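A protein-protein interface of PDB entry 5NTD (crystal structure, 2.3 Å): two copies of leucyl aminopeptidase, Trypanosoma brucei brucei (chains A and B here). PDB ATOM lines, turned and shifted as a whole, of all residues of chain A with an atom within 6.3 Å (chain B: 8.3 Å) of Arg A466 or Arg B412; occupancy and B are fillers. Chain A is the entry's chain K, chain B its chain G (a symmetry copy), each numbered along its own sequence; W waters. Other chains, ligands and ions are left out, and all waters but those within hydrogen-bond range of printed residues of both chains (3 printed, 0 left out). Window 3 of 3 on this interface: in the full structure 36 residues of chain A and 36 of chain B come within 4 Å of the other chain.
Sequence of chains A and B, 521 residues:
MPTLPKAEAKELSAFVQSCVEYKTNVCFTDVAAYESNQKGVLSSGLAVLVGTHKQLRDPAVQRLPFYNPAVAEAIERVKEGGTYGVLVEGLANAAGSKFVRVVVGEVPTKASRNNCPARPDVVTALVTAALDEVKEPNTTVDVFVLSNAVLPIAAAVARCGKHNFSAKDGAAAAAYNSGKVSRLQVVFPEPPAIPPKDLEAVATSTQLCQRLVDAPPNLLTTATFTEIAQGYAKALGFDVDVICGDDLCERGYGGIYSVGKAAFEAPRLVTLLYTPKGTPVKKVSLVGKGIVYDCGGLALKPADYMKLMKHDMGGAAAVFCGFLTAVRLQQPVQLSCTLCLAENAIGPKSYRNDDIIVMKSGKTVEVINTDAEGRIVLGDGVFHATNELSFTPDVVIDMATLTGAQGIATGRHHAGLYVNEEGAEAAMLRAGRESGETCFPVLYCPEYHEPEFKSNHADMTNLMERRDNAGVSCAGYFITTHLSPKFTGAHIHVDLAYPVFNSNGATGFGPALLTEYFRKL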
ATOM      1  N   TYR A 448      26.368 -13.348  19.505  1.00  0.00           N
ATOM      2  CA  TYR A 448      26.076 -13.606  18.073  1.00  0.00           C
ATOM      3  C   TYR A 448      27.316 -13.699  17.179  1.00  0.00           C
ATOM      4  O   TYR A 448      27.253 -14.237  16.094  1.00  0.00           O
ATOM      5  CB  TYR A 448      25.101 -12.581  17.509  1.00  0.00           C
ATOM      6  CG  TYR A 448      23.690 -12.617  18.080  1.00  0.00           C
ATOM      7  CD1 TYR A 448      23.232 -13.687  18.864  1.00  0.00           C
ATOM      8  CD2 TYR A 448      22.806 -11.579  17.817  1.00  0.00           C
ATOM      9  CE1 TYR A 448      21.945 -13.713  19.372  1.00  0.00           C
ATOM     10  CE2 TYR A 448      21.525 -11.607  18.324  1.00  0.00           C
ATOM     11  CZ  TYR A 448      21.093 -12.669  19.098  1.00  0.00           C
ATOM     12  OH  TYR A 448      19.829 -12.679  19.615  1.00  0.00           O
ATOM     13  N   GLU A 452      30.340 -17.663  14.758  1.00  0.00           N
ATOM     14  CA  GLU A 452      30.907 -17.491  13.401  1.00  0.00           C
ATOM     15  C   GLU A 452      32.330 -18.001  13.291  1.00  0.00           C
ATOM     16  O   GLU A 452      32.821 -18.230  12.198  1.00  0.00           O
ATOM     17  CB  GLU A 452      30.868 -16.034  12.950  1.00  0.00           C
ATOM     18  CG  GLU A 452      29.465 -15.522  12.718  1.00  0.00           C
ATOM     19  CD  GLU A 452      28.758 -16.187  11.541  1.00  0.00           C
ATOM     20  OE1 GLU A 452      29.434 -16.849  10.749  1.00  0.00           O
ATOM     21  OE2 GLU A 452      27.542 -16.030  11.428  1.00  0.00           O
ATOM     22  N   LEU A 463      38.186 -16.257  10.539  1.00  0.00           N
ATOM     23  CA  LEU A 463      37.228 -15.715   9.605  1.00  0.00           C
ATOM     24  C   LEU A 463      35.874 -16.285   9.837  1.00  0.00           C
ATOM     25  O   LEU A 463      35.697 -17.461   9.976  1.00  0.00           O
ATOM     26  CB  LEU A 463      37.646 -15.955   8.137  1.00  0.00           C
ATOM     27  CG  LEU A 463      36.834 -15.190   7.078  1.00  0.00           C
ATOM     28  CD1 LEU A 463      37.166 -13.711   7.106  1.00  0.00           C
ATOM     29  CD2 LEU A 463      37.086 -15.707   5.673  1.00  0.00           C
ATOM     30  N   MET A 464      34.906 -15.419   9.739  1.00  0.00           N
ATOM     31  CA  MET A 464      33.491 -15.778   9.883  1.00  0.00           C
ATOM     32  C   MET A 464      33.049 -16.793   8.826  1.00  0.00           C
ATOM     33  O   MET A 464      33.344 -16.640   7.667  1.00  0.00           O
ATOM     34  CB  MET A 464      32.589 -14.553   9.764  1.00  0.00           C
ATOM     35  CG  MET A 464      32.968 -13.417  10.680  1.00  0.00           C
ATOM     36  SD  MET A 464      32.951 -11.893   9.712  1.00  0.00           S
ATOM     37  CE  MET A 464      31.183 -11.498   9.708  1.00  0.00           C
ATOM     38  N   GLU A 465      32.305 -17.789   9.263  1.00  0.00           N
ATOM     39  CA  GLU A 465      31.606 -18.731   8.352  1.00  0.00           C
ATOM     40  C   GLU A 465      30.669 -17.959   7.404  1.00  0.00           C
ATOM     41  O   GLU A 465      30.667 -18.180   6.216  1.00  0.00           O
ATOM     42  CB  GLU A 465      30.830 -19.779   9.155  1.00  0.00           C
ATOM     43  CG  GLU A 465      30.022 -20.809   8.362  1.00  0.00           C
ATOM     44  CD  GLU A 465      30.829 -21.540   7.288  1.00  0.00           C
ATOM     45  OE1 GLU A 465      32.065 -21.692   7.429  1.00  0.00           O
ATOM     46  OE2 GLU A 465      30.238 -21.997   6.289  1.00  0.00           O
ATOM     47  N   ARG A 466      29.936 -16.996   7.957  1.00  0.00           N
ATOM     48  CA  ARG A 466      29.051 -16.110   7.175  1.00  0.00           C
ATOM     49  C   ARG A 466      29.531 -14.664   7.246  1.00  0.00           C
ATOM     50  O   ARG A 466      29.533 -14.059   8.318  1.00  0.00           O
ATOM     51  CB  ARG A 466      27.620 -16.201   7.681  1.00  0.00           C
ATOM     52  CG  ARG A 466      27.090 -17.622   7.764  1.00  0.00           C
ATOM     53  CD  ARG A 466      25.683 -17.712   8.343  1.00  0.00           C
ATOM     54  NE  ARG A 466      25.612 -17.263   9.726  1.00  0.00           N
ATOM     55  CZ  ARG A 466      24.506 -17.252  10.479  1.00  0.00           C
ATOM     56  NH1 ARG A 466      23.356 -17.711  10.011  1.00  0.00           N
ATOM     57  NH2 ARG A 466      24.551 -16.774  11.718  1.00  0.00           N
ATOM     58  N   ARG A 467      29.908 -14.116   6.106  1.00  0.00           N
ATOM     59  CA  ARG A 467      30.541 -12.764   6.027  1.00  0.00           C
ATOM     60  C   ARG A 467      29.497 -11.625   6.058  1.00  0.00           C
ATOM     61  O   ARG A 467      29.828 -10.457   6.253  1.00  0.00           O
ATOM     62  CB  ARG A 467      31.482 -12.640   4.798  1.00  0.00           C
ATOM     63  N   ASP A 468      28.239 -12.005   5.937  1.00  0.00           N
ATOM     64  CA  ASP A 468      27.118 -11.061   6.009  1.00  0.00           C
ATOM     65  C   ASP A 468      26.407 -11.012   7.377  1.00  0.00           C
ATOM     66  O   ASP A 468      25.198 -10.869   7.487  1.00  0.00           O
ATOM     67  CB  ASP A 468      26.109 -11.367   4.910  1.00  0.00           C
ATOM     68  CG  ASP A 468      25.616 -12.801   4.932  1.00  0.00           C
ATOM     69  OD1 ASP A 468      25.764 -13.520   5.947  1.00  0.00           O
ATOM     70  OD2 ASP A 468      25.068 -13.197   3.899  1.00  0.00           O
ATOM     71  N   ASN A 469      27.196 -11.152   8.418  1.00  0.00           N
ATOM     72  CA  ASN A 469      26.704 -11.173   9.830  1.00  0.00           C
ATOM     73  C   ASN A 469      27.516 -10.265  10.786  1.00  0.00           C
ATOM     74  O   ASN A 469      28.143 -10.730  11.718  1.00  0.00           O
ATOM     75  CB  ASN A 469      26.680 -12.596  10.357  1.00  0.00           C
ATOM     76  CG  ASN A 469      25.844 -12.733  11.613  1.00  0.00           C
ATOM     77  OD1 ASN A 469      25.015 -11.875  11.923  1.00  0.00           O
ATOM     78  ND2 ASN A 469      26.082 -13.787  12.352  1.00  0.00           N
ATOM     79  N   ALA A 470      27.490  -8.978  10.467  1.00  0.00           N
ATOM     80  CA  ALA A 470      28.162  -7.918  11.247  1.00  0.00           C
ATOM     81  C   ALA A 470      29.672  -8.121  11.213  1.00  0.00           C
ATOM     82  O   ALA A 470      30.315  -8.442  12.181  1.00  0.00           O
ATOM     83  CB  ALA A 470      27.656  -7.888  12.673  1.00  0.00           C
ATOM     84  N   CYS A 474      32.434  -8.622  14.125  1.00  0.00           N
ATOM     85  CA  CYS A 474      33.047  -9.961  14.248  1.00  0.00           C
ATOM     86  C   CYS A 474      34.571  -9.878  14.290  1.00  0.00           C
ATOM     87  O   CYS A 474      35.217 -10.588  15.047  1.00  0.00           O
ATOM     88  CB  CYS A 474      32.585 -10.907  13.161  1.00  0.00           C
ATOM     89  SG  CYS A 474      30.918 -11.550  13.427  1.00  0.00           S
ATOM     90  N   LEU B 308      15.599 -16.689  -2.750  1.00  0.00           N
ATOM     91  CA  LEU B 308      15.146 -15.990  -1.515  1.00  0.00           C
ATOM     92  C   LEU B 308      14.749 -14.504  -1.664  1.00  0.00           C
ATOM     93  O   LEU B 308      14.381 -13.876  -0.683  1.00  0.00           O
ATOM     94  CB  LEU B 308      16.165 -16.187  -0.373  1.00  0.00           C
ATOM     95  CG  LEU B 308      16.447 -17.683  -0.021  1.00  0.00           C
ATOM     96  CD1 LEU B 308      17.351 -17.778   1.209  1.00  0.00           C
ATOM     97  CD2 LEU B 308      15.184 -18.573   0.143  1.00  0.00           C
ATOM     98  N   GLN B 406      23.258  -4.103   4.954  1.00  0.00           N
ATOM     99  CA  GLN B 406      22.657  -4.242   6.274  1.00  0.00           C
ATOM    100  C   GLN B 406      23.227  -5.444   7.005  1.00  0.00           C
ATOM    101  O   GLN B 406      23.596  -5.371   8.168  1.00  0.00           O
ATOM    102  CB  GLN B 406      21.145  -4.358   6.167  1.00  0.00           C
ATOM    103  CG  GLN B 406      20.443  -4.492   7.503  1.00  0.00           C
ATOM    104  CD  GLN B 406      20.285  -5.919   7.954  1.00  0.00           C
ATOM    105  OE1 GLN B 406      19.665  -6.741   7.276  1.00  0.00           O
ATOM    106  NE2 GLN B 406      20.928  -6.256   9.065  1.00  0.00           N
ATOM    107  N   GLY B 407      23.308  -6.567   6.309  1.00  0.00           N
ATOM    108  CA  GLY B 407      23.864  -7.784   6.902  1.00  0.00           C
ATOM    109  C   GLY B 407      25.316  -7.581   7.335  1.00  0.00           C
ATOM    110  O   GLY B 407      25.751  -8.006   8.391  1.00  0.00           O
ATOM    111  N   ILE B 408      26.062  -6.963   6.462  1.00  0.00           N
ATOM    112  CA  ILE B 408      27.484  -6.685   6.713  1.00  0.00           C
ATOM    113  C   ILE B 408      27.662  -5.771   7.909  1.00  0.00           C
ATOM    114  O   ILE B 408      28.545  -5.962   8.734  1.00  0.00           O
ATOM    115  CB  ILE B 408      28.150  -6.077   5.449  1.00  0.00           C
ATOM    116  CG1 ILE B 408      28.244  -7.173   4.353  1.00  0.00           C
ATOM    117  CG2 ILE B 408      29.526  -5.526   5.766  1.00  0.00           C
ATOM    118  CD1 ILE B 408      28.583  -6.644   2.988  1.00  0.00           C
ATOM    119  N   ALA B 409      26.789  -4.799   7.992  1.00  0.00           N
ATOM    120  CA  ALA B 409      26.876  -3.778   9.042  1.00  0.00           C
ATOM    121  C   ALA B 409      26.367  -4.250  10.414  1.00  0.00           C
ATOM    122  O   ALA B 409      27.088  -4.184  11.406  1.00  0.00           O
ATOM    123  CB  ALA B 409      26.142  -2.508   8.615  1.00  0.00           C
ATOM    124  N   THR B 410      25.115  -4.649  10.450  1.00  0.00           N
ATOM    125  CA  THR B 410      24.409  -4.991  11.725  1.00  0.00           C
ATOM    126  C   THR B 410      24.026  -6.456  11.897  1.00  0.00           C
ATOM    127  O   THR B 410      23.594  -6.883  12.957  1.00  0.00           O
ATOM    128  CB  THR B 410      23.154  -4.134  11.964  1.00  0.00           C
ATOM    129  OG1 THR B 410      22.155  -4.424  10.987  1.00  0.00           O
ATOM    130  CG2 THR B 410      23.492  -2.671  11.911  1.00  0.00           C
ATOM    131  N   GLY B 411      24.207  -7.238  10.855  1.00  0.00           N
ATOM    132  CA  GLY B 411      24.135  -8.724  10.973  1.00  0.00           C
ATOM    133  C   GLY B 411      22.764  -9.339  10.804  1.00  0.00           C
ATOM    134  O   GLY B 411      21.802  -8.669  10.439  1.00  0.00           O
ATOM    135  N   ARG B 412      22.689 -10.625  11.096  1.00  0.00           N
ATOM    136  CA  ARG B 412      21.495 -11.416  10.767  1.00  0.00           C
ATOM    137  C   ARG B 412      20.334 -11.221  11.742  1.00  0.00           C
ATOM    138  O   ARG B 412      19.208 -11.508  11.408  1.00  0.00           O
ATOM    139  CB  ARG B 412      21.849 -12.917  10.670  1.00  0.00           C
ATOM    140  CG  ARG B 412      22.968 -13.309   9.704  1.00  0.00           C
ATOM    141  CD  ARG B 412      22.457 -13.152   8.326  1.00  0.00           C
ATOM    142  NE  ARG B 412      23.289 -13.780   7.309  1.00  0.00           N
ATOM    143  CZ  ARG B 412      22.971 -14.882   6.633  1.00  0.00           C
ATOM    144  NH1 ARG B 412      21.823 -15.531   6.846  1.00  0.00           N
ATOM    145  NH2 ARG B 412      23.826 -15.345   5.737  1.00  0.00           N
ATOM    146  N   HIS B 413      20.623 -10.705  12.933  1.00  0.00           N
ATOM    147  CA  HIS B 413      19.625 -10.611  14.012  1.00  0.00           C
ATOM    148  C   HIS B 413      19.188  -9.227  14.366  1.00  0.00           C
ATOM    149  O   HIS B 413      18.236  -9.057  15.096  1.00  0.00           O
ATOM    150  CB  HIS B 413      20.105 -11.316  15.279  1.00  0.00           C
ATOM    151  CG  HIS B 413      20.576 -12.703  15.022  1.00  0.00           C
ATOM    152  ND1 HIS B 413      21.868 -12.981  14.634  1.00  0.00           N
ATOM    153  CD2 HIS B 413      19.921 -13.885  15.028  1.00  0.00           C
ATOM    154  CE1 HIS B 413      21.995 -14.278  14.436  1.00  0.00           C
ATOM    155  NE2 HIS B 413      20.829 -14.848  14.667  1.00  0.00           N
ATOM    156  N   HIS B 414      19.912  -8.252  13.883  1.00  0.00           N
ATOM    157  CA  HIS B 414      19.632  -6.859  14.204  1.00  0.00           C
ATOM    158  C   HIS B 414      19.328  -6.059  12.946  1.00  0.00           C
ATOM    159  O   HIS B 414      20.209  -5.878  12.103  1.00  0.00           O
ATOM    160  CB  HIS B 414      20.818  -6.199  14.895  1.00  0.00           C
ATOM    161  CG  HIS B 414      21.068  -6.696  16.280  1.00  0.00           C
ATOM    162  ND1 HIS B 414      21.670  -7.906  16.542  1.00  0.00           N
ATOM    163  CD2 HIS B 414      20.802  -6.139  17.476  1.00  0.00           C
ATOM    164  CE1 HIS B 414      21.760  -8.068  17.841  1.00  0.00           C
ATOM    165  NE2 HIS B 414      21.233  -7.017  18.430  1.00  0.00           N
ATOM    166  N   ALA B 415      18.102  -5.570  12.851  1.00  0.00           N
ATOM    167  CA  ALA B 415      17.729  -4.671  11.783  1.00  0.00           C
ATOM    168  C   ALA B 415      18.458  -3.350  11.967  1.00  0.00           C
ATOM    169  O   ALA B 415      18.645  -2.863  13.080  1.00  0.00           O
ATOM    170  CB  ALA B 415      16.239  -4.437  11.771  1.00  0.00           C
ATOM    171  N   THR B 438      15.313  -7.466  17.590  1.00  0.00           N
ATOM    172  CA  THR B 438      16.365  -6.492  17.922  1.00  0.00           C
ATOM    173  C   THR B 438      16.815  -5.657  16.718  1.00  0.00           C
ATOM    174  O   THR B 438      16.755  -6.109  15.606  1.00  0.00           O
ATOM    175  CB  THR B 438      17.607  -7.161  18.519  1.00  0.00           C
ATOM    176  OG1 THR B 438      17.945  -8.293  17.727  1.00  0.00           O
ATOM    177  CG2 THR B 438      17.339  -7.619  19.929  1.00  0.00           C
ATOM    178  N   LEU B 496      15.716  -4.287   7.253  1.00  0.00           N
ATOM    179  CA  LEU B 496      15.604  -5.650   7.831  1.00  0.00           C
ATOM    180  C   LEU B 496      15.825  -6.778   6.807  1.00  0.00           C
ATOM    181  O   LEU B 496      15.238  -7.845   6.873  1.00  0.00           O
ATOM    182  CB  LEU B 496      14.271  -5.838   8.564  1.00  0.00           C
ATOM    183  CG  LEU B 496      13.026  -5.181   7.976  1.00  0.00           C
ATOM    184  CD1 LEU B 496      12.690  -5.725   6.605  1.00  0.00           C
ATOM    185  CD2 LEU B 496      11.860  -5.420   8.915  1.00  0.00           C
ATOM    186  N   ALA B 497      16.745  -6.506   5.905  1.00  0.00           N
ATOM    187  CA  ALA B 497      17.109  -7.457   4.828  1.00  0.00           C
ATOM    188  C   ALA B 497      17.312  -8.871   5.342  1.00  0.00           C
ATOM    189  O   ALA B 497      16.772  -9.821   4.820  1.00  0.00           O
ATOM    190  CB  ALA B 497      18.339  -6.973   4.063  1.00  0.00           C
ATOM    191  N   TYR B 498      18.108  -8.995   6.376  1.00  0.00           N
ATOM    192  CA  TYR B 498      18.470 -10.317   6.936  1.00  0.00           C
ATOM    193  C   TYR B 498      17.627 -10.839   8.124  1.00  0.00           C
ATOM    194  O   TYR B 498      17.357 -12.027   8.193  1.00  0.00           O
ATOM    195  CB  TYR B 498      19.962 -10.382   7.259  1.00  0.00           C
ATOM    196  CG  TYR B 498      20.818 -10.421   6.018  1.00  0.00           C
ATOM    197  CD1 TYR B 498      21.192  -9.251   5.379  1.00  0.00           C
ATOM    198  CD2 TYR B 498      21.225 -11.636   5.472  1.00  0.00           C
ATOM    199  CE1 TYR B 498      21.958  -9.280   4.235  1.00  0.00           C
ATOM    200  CE2 TYR B 498      21.999 -11.676   4.337  1.00  0.00           C
ATOM    201  CZ  TYR B 498      22.359 -10.491   3.722  1.00  0.00           C
ATOM    202  OH  TYR B 498      23.116 -10.530   2.571  1.00  0.00           O
ATOM    203  N   PRO B 499      17.184  -9.962   9.023  1.00  0.00           N
ATOM    204  CA  PRO B 499      16.430 -10.484  10.138  1.00  0.00           C
ATOM    205  C   PRO B 499      15.084 -11.143   9.807  1.00  0.00           C
ATOM    206  O   PRO B 499      14.523 -11.841  10.636  1.00  0.00           O
ATOM    207  CB  PRO B 499      16.223  -9.239  11.002  1.00  0.00           C
ATOM    208  CG  PRO B 499      17.452  -8.425  10.757  1.00  0.00           C
ATOM    209  CD  PRO B 499      17.697  -8.613   9.295  1.00  0.00           C
ATOM    210  N   VAL B 500      14.568 -10.872   8.610  1.00  0.00           N
ATOM    211  CA  VAL B 500      13.299 -11.471   8.172  1.00  0.00           C
ATOM    212  C   VAL B 500      13.365 -12.955   7.846  1.00  0.00           C
ATOM    213  O   VAL B 500      12.349 -13.575   7.572  1.00  0.00           O
ATOM    214  CB  VAL B 500      12.645 -10.742   6.997  1.00  0.00           C
ATOM    215  CG1 VAL B 500      12.333  -9.319   7.396  1.00  0.00           C
ATOM    216  CG2 VAL B 500      13.487 -10.813   5.733  1.00  0.00           C
ATOM    217  N   PHE B 501      14.552 -13.522   7.842  1.00  0.00           N
ATOM    218  CA  PHE B 501      14.704 -14.950   7.499  1.00  0.00           C
ATOM    219  C   PHE B 501      15.894 -15.609   8.200  1.00  0.00           C
ATOM    220  O   PHE B 501      16.797 -14.963   8.655  1.00  0.00           O
ATOM    221  CB  PHE B 501      14.782 -15.170   5.973  1.00  0.00           C
ATOM    222  CG  PHE B 501      16.135 -14.861   5.362  1.00  0.00           C
ATOM    223  CD1 PHE B 501      16.489 -13.573   5.028  1.00  0.00           C
ATOM    224  CD2 PHE B 501      17.063 -15.882   5.143  1.00  0.00           C
ATOM    225  CE1 PHE B 501      17.741 -13.282   4.515  1.00  0.00           C
ATOM    226  CE2 PHE B 501      18.317 -15.598   4.620  1.00  0.00           C
ATOM    227  CZ  PHE B 501      18.650 -14.295   4.293  1.00  0.00           C
ATOM    228  N   ASN B 502      15.834 -16.920   8.256  1.00  0.00           N
ATOM    229  CA  ASN B 502      16.965 -17.722   8.636  1.00  0.00           C
ATOM    230  C   ASN B 502      16.955 -18.979   7.766  1.00  0.00           C
ATOM    231  O   ASN B 502      16.249 -19.045   6.802  1.00  0.00           O
ATOM    232  CB  ASN B 502      16.949 -18.024  10.139  1.00  0.00           C
ATOM    233  CG  ASN B 502      15.753 -18.873  10.571  1.00  0.00           C
ATOM    234  OD1 ASN B 502      15.148 -19.606   9.791  1.00  0.00           O
ATOM    235  ND2 ASN B 502      15.443 -18.797  11.835  1.00  0.00           N
ATOM    236  N   SER B 503      17.719 -19.981   8.146  1.00  0.00           N
ATOM    237  CA  SER B 503      17.919 -21.152   7.288  1.00  0.00           C
ATOM    238  C   SER B 503      16.674 -22.046   7.213  1.00  0.00           C
ATOM    239  O   SER B 503      16.559 -22.849   6.315  1.00  0.00           O
ATOM    240  CB  SER B 503      19.125 -21.977   7.712  1.00  0.00           C
ATOM    241  OG  SER B 503      18.867 -22.519   8.981  1.00  0.00           O
ATOM    242  N   THR B 507      11.100 -15.533   9.443  1.00  0.00           N
ATOM    243  CA  THR B 507      11.107 -15.417  10.910  1.00  0.00           C
ATOM    244  C   THR B 507       9.858 -14.711  11.462  1.00  0.00           C
ATOM    245  O   THR B 507       9.610 -14.739  12.645  1.00  0.00           O
ATOM    246  CB  THR B 507      12.329 -14.613  11.407  1.00  0.00           C
ATOM    247  OG1 THR B 507      12.359 -13.357  10.725  1.00  0.00           O
ATOM    248  CG2 THR B 507      13.576 -15.353  11.158  1.00  0.00           C
ATOM    249  N   PHE B 509       9.784 -11.535  11.608  1.00  0.00           N
ATOM    250  CA  PHE B 509      10.371 -10.347  12.266  1.00  0.00           C
ATOM    251  C   PHE B 509       9.691  -9.081  11.781  1.00  0.00           C
ATOM    252  O   PHE B 509       9.497  -8.885  10.588  1.00  0.00           O
ATOM    253  CB  PHE B 509      11.872 -10.279  11.951  1.00  0.00           C
ATOM    254  CG  PHE B 509      12.616  -9.133  12.585  1.00  0.00           C
ATOM    255  CD1 PHE B 509      12.519  -7.838  12.075  1.00  0.00           C
ATOM    256  CD2 PHE B 509      13.512  -9.369  13.607  1.00  0.00           C
ATOM    257  CE1 PHE B 509      13.261  -6.803  12.618  1.00  0.00           C
ATOM    258  CE2 PHE B 509      14.247  -8.341  14.159  1.00  0.00           C
ATOM    259  CZ  PHE B 509      14.127  -7.063  13.666  1.00  0.00           C
HETATM  260  O   HOH W   1      18.234 -10.986  18.452  1.00  0.00           O
HETATM  261  O   HOH W   2      29.672  -5.048  12.194  1.00  0.00           O
HETATM  262  O   HOH W   3      24.298 -11.338  14.548  1.00  0.00           O
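Water W1 lies within hydrogen-bond range of the side-chain hydroxyl (OH) of Tyr A448 (2.6 Å) and the side-chain hydroxyl (OG1) of Thr B438 (2.8 Å).
Water W3 lies within hydrogen-bond range of OD1 of Asn A469 (2.8 Å) and ND1 of His B413 (2.9 Å).
Water W2 bridges the backbone carbonyl oxygen (O) of Ala B409 and the backbone carbonyl oxygen (O) of Ala A470.
OE1 of Gln B406 is in hydrogen-bond range of N of Tyr B498 (2.9 Å).
The backbone carbonyl oxygen of Ala A470 sits at hydrogen-bond distance from the side-chain sulfur of Cys A474 (3.4 Å).
The side-chain hydroxyl (OG1) of Thr B410 is in hydrogen-bond range of the side-chain amide nitrogen (NE2) of Gln B406 (2.9 Å).
The side-chain carboxylate of Glu A452 lies within salt-bridge range of the guanidinium group of Arg A466 (2.9 Å).
O of Asn A469 is in hydrogen-bond range of SG of Cys A474, 3.4 Å away.
OG1 of Thr B438 sits at hydrogen-bond distance from O of His B413 (2.8 Å).
Among the printed residues, pairs that only touch across the chains: Ala A470 with Ile B408 (3.2 Å), Tyr A448 with His B413 (3.4 Å), Ala A470 with Gly B411 (3.4 Å), Asn A469 with Gly B411 (3.4 Å), Asp A468 with Tyr B498 (3.5 Å), Tyr A448 with His B414 (3.6 Å), Ala A470 with Ala B409 (3.9 Å), Ala A470 with Thr B410 (3.98 Å) and Arg A466 with Arg B412 (3.98 Å).
The guanidinium group (NH2) of Arg B412 lies within salt-bridge range of the side-chain carboxylate (OD1) of Asp A468.
The backbone NH (N) of Ala A470 sits at hydrogen-bond distance from the backbone carbonyl oxygen (O) of Gly B407, at 2.9 Å.
The side-chain amide oxygen of Asn A469 sits at hydrogen-bond distance from the backbone NH of Arg B412 (2.8 Å).
The backbone carbonyl oxygen (O) of Asp A468 sits close to the backbone carbonyl oxygen (O) of Gly B407 (3.1 Å).
The backbone carbonyl oxygen (O) of Gly B407 lies within hydrogen-bond range of the backbone NH (N) of Asn A469, 3.5 Å away.
No position is printed for both chains.
Of the 14 pairs that touch across the chains among the printed residues, none has its exchanged pair printed and touching as well.
Of the 22 printed residues of chain B, 9 touch a printed residue of chain A.
Of the 11 printed residues of chain A, 5 touch a printed residue of chain B.
Printed residues of chain A that touch a printed residue of chain B: Tyr A448, Arg A466, Asp A468, Asn A469 and Ala A470.
Hydrophobic or aromatic side chains of chain A within 4 Å of the printed part of chain B: Tyr A448 and Ala A470.
Printed residues of chain B within 4 Å of Tyr A448: His B413 and His B414.
Leu A463 touches none of the printed residues of chain B.
Printed residues of chain B within 4 Å of Arg A466: Arg B412.
No residue of chain B comes within 4 Å of Arg A467.
Of the printed residues of chain B, Ala A470 touches Gly B407 (2.9 Å), Ile B408 (3.2 Å), Ala B409 (3.9 Å), Thr B410 (3.98 Å) and Gly B411 (3.4 Å).
Of the printed residues of chain A, Gly B407 touches Asp A468, Asn A469 and Ala A470.
Of the printed residues of chain A, Arg B412 touches Arg A466, Asp A468 and Asn A469.
Ser B503 touches none of the printed residues of chain A.
The nearest printed residue of chain B that does not touch Asn A469 is His B413 (4.3 Å).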
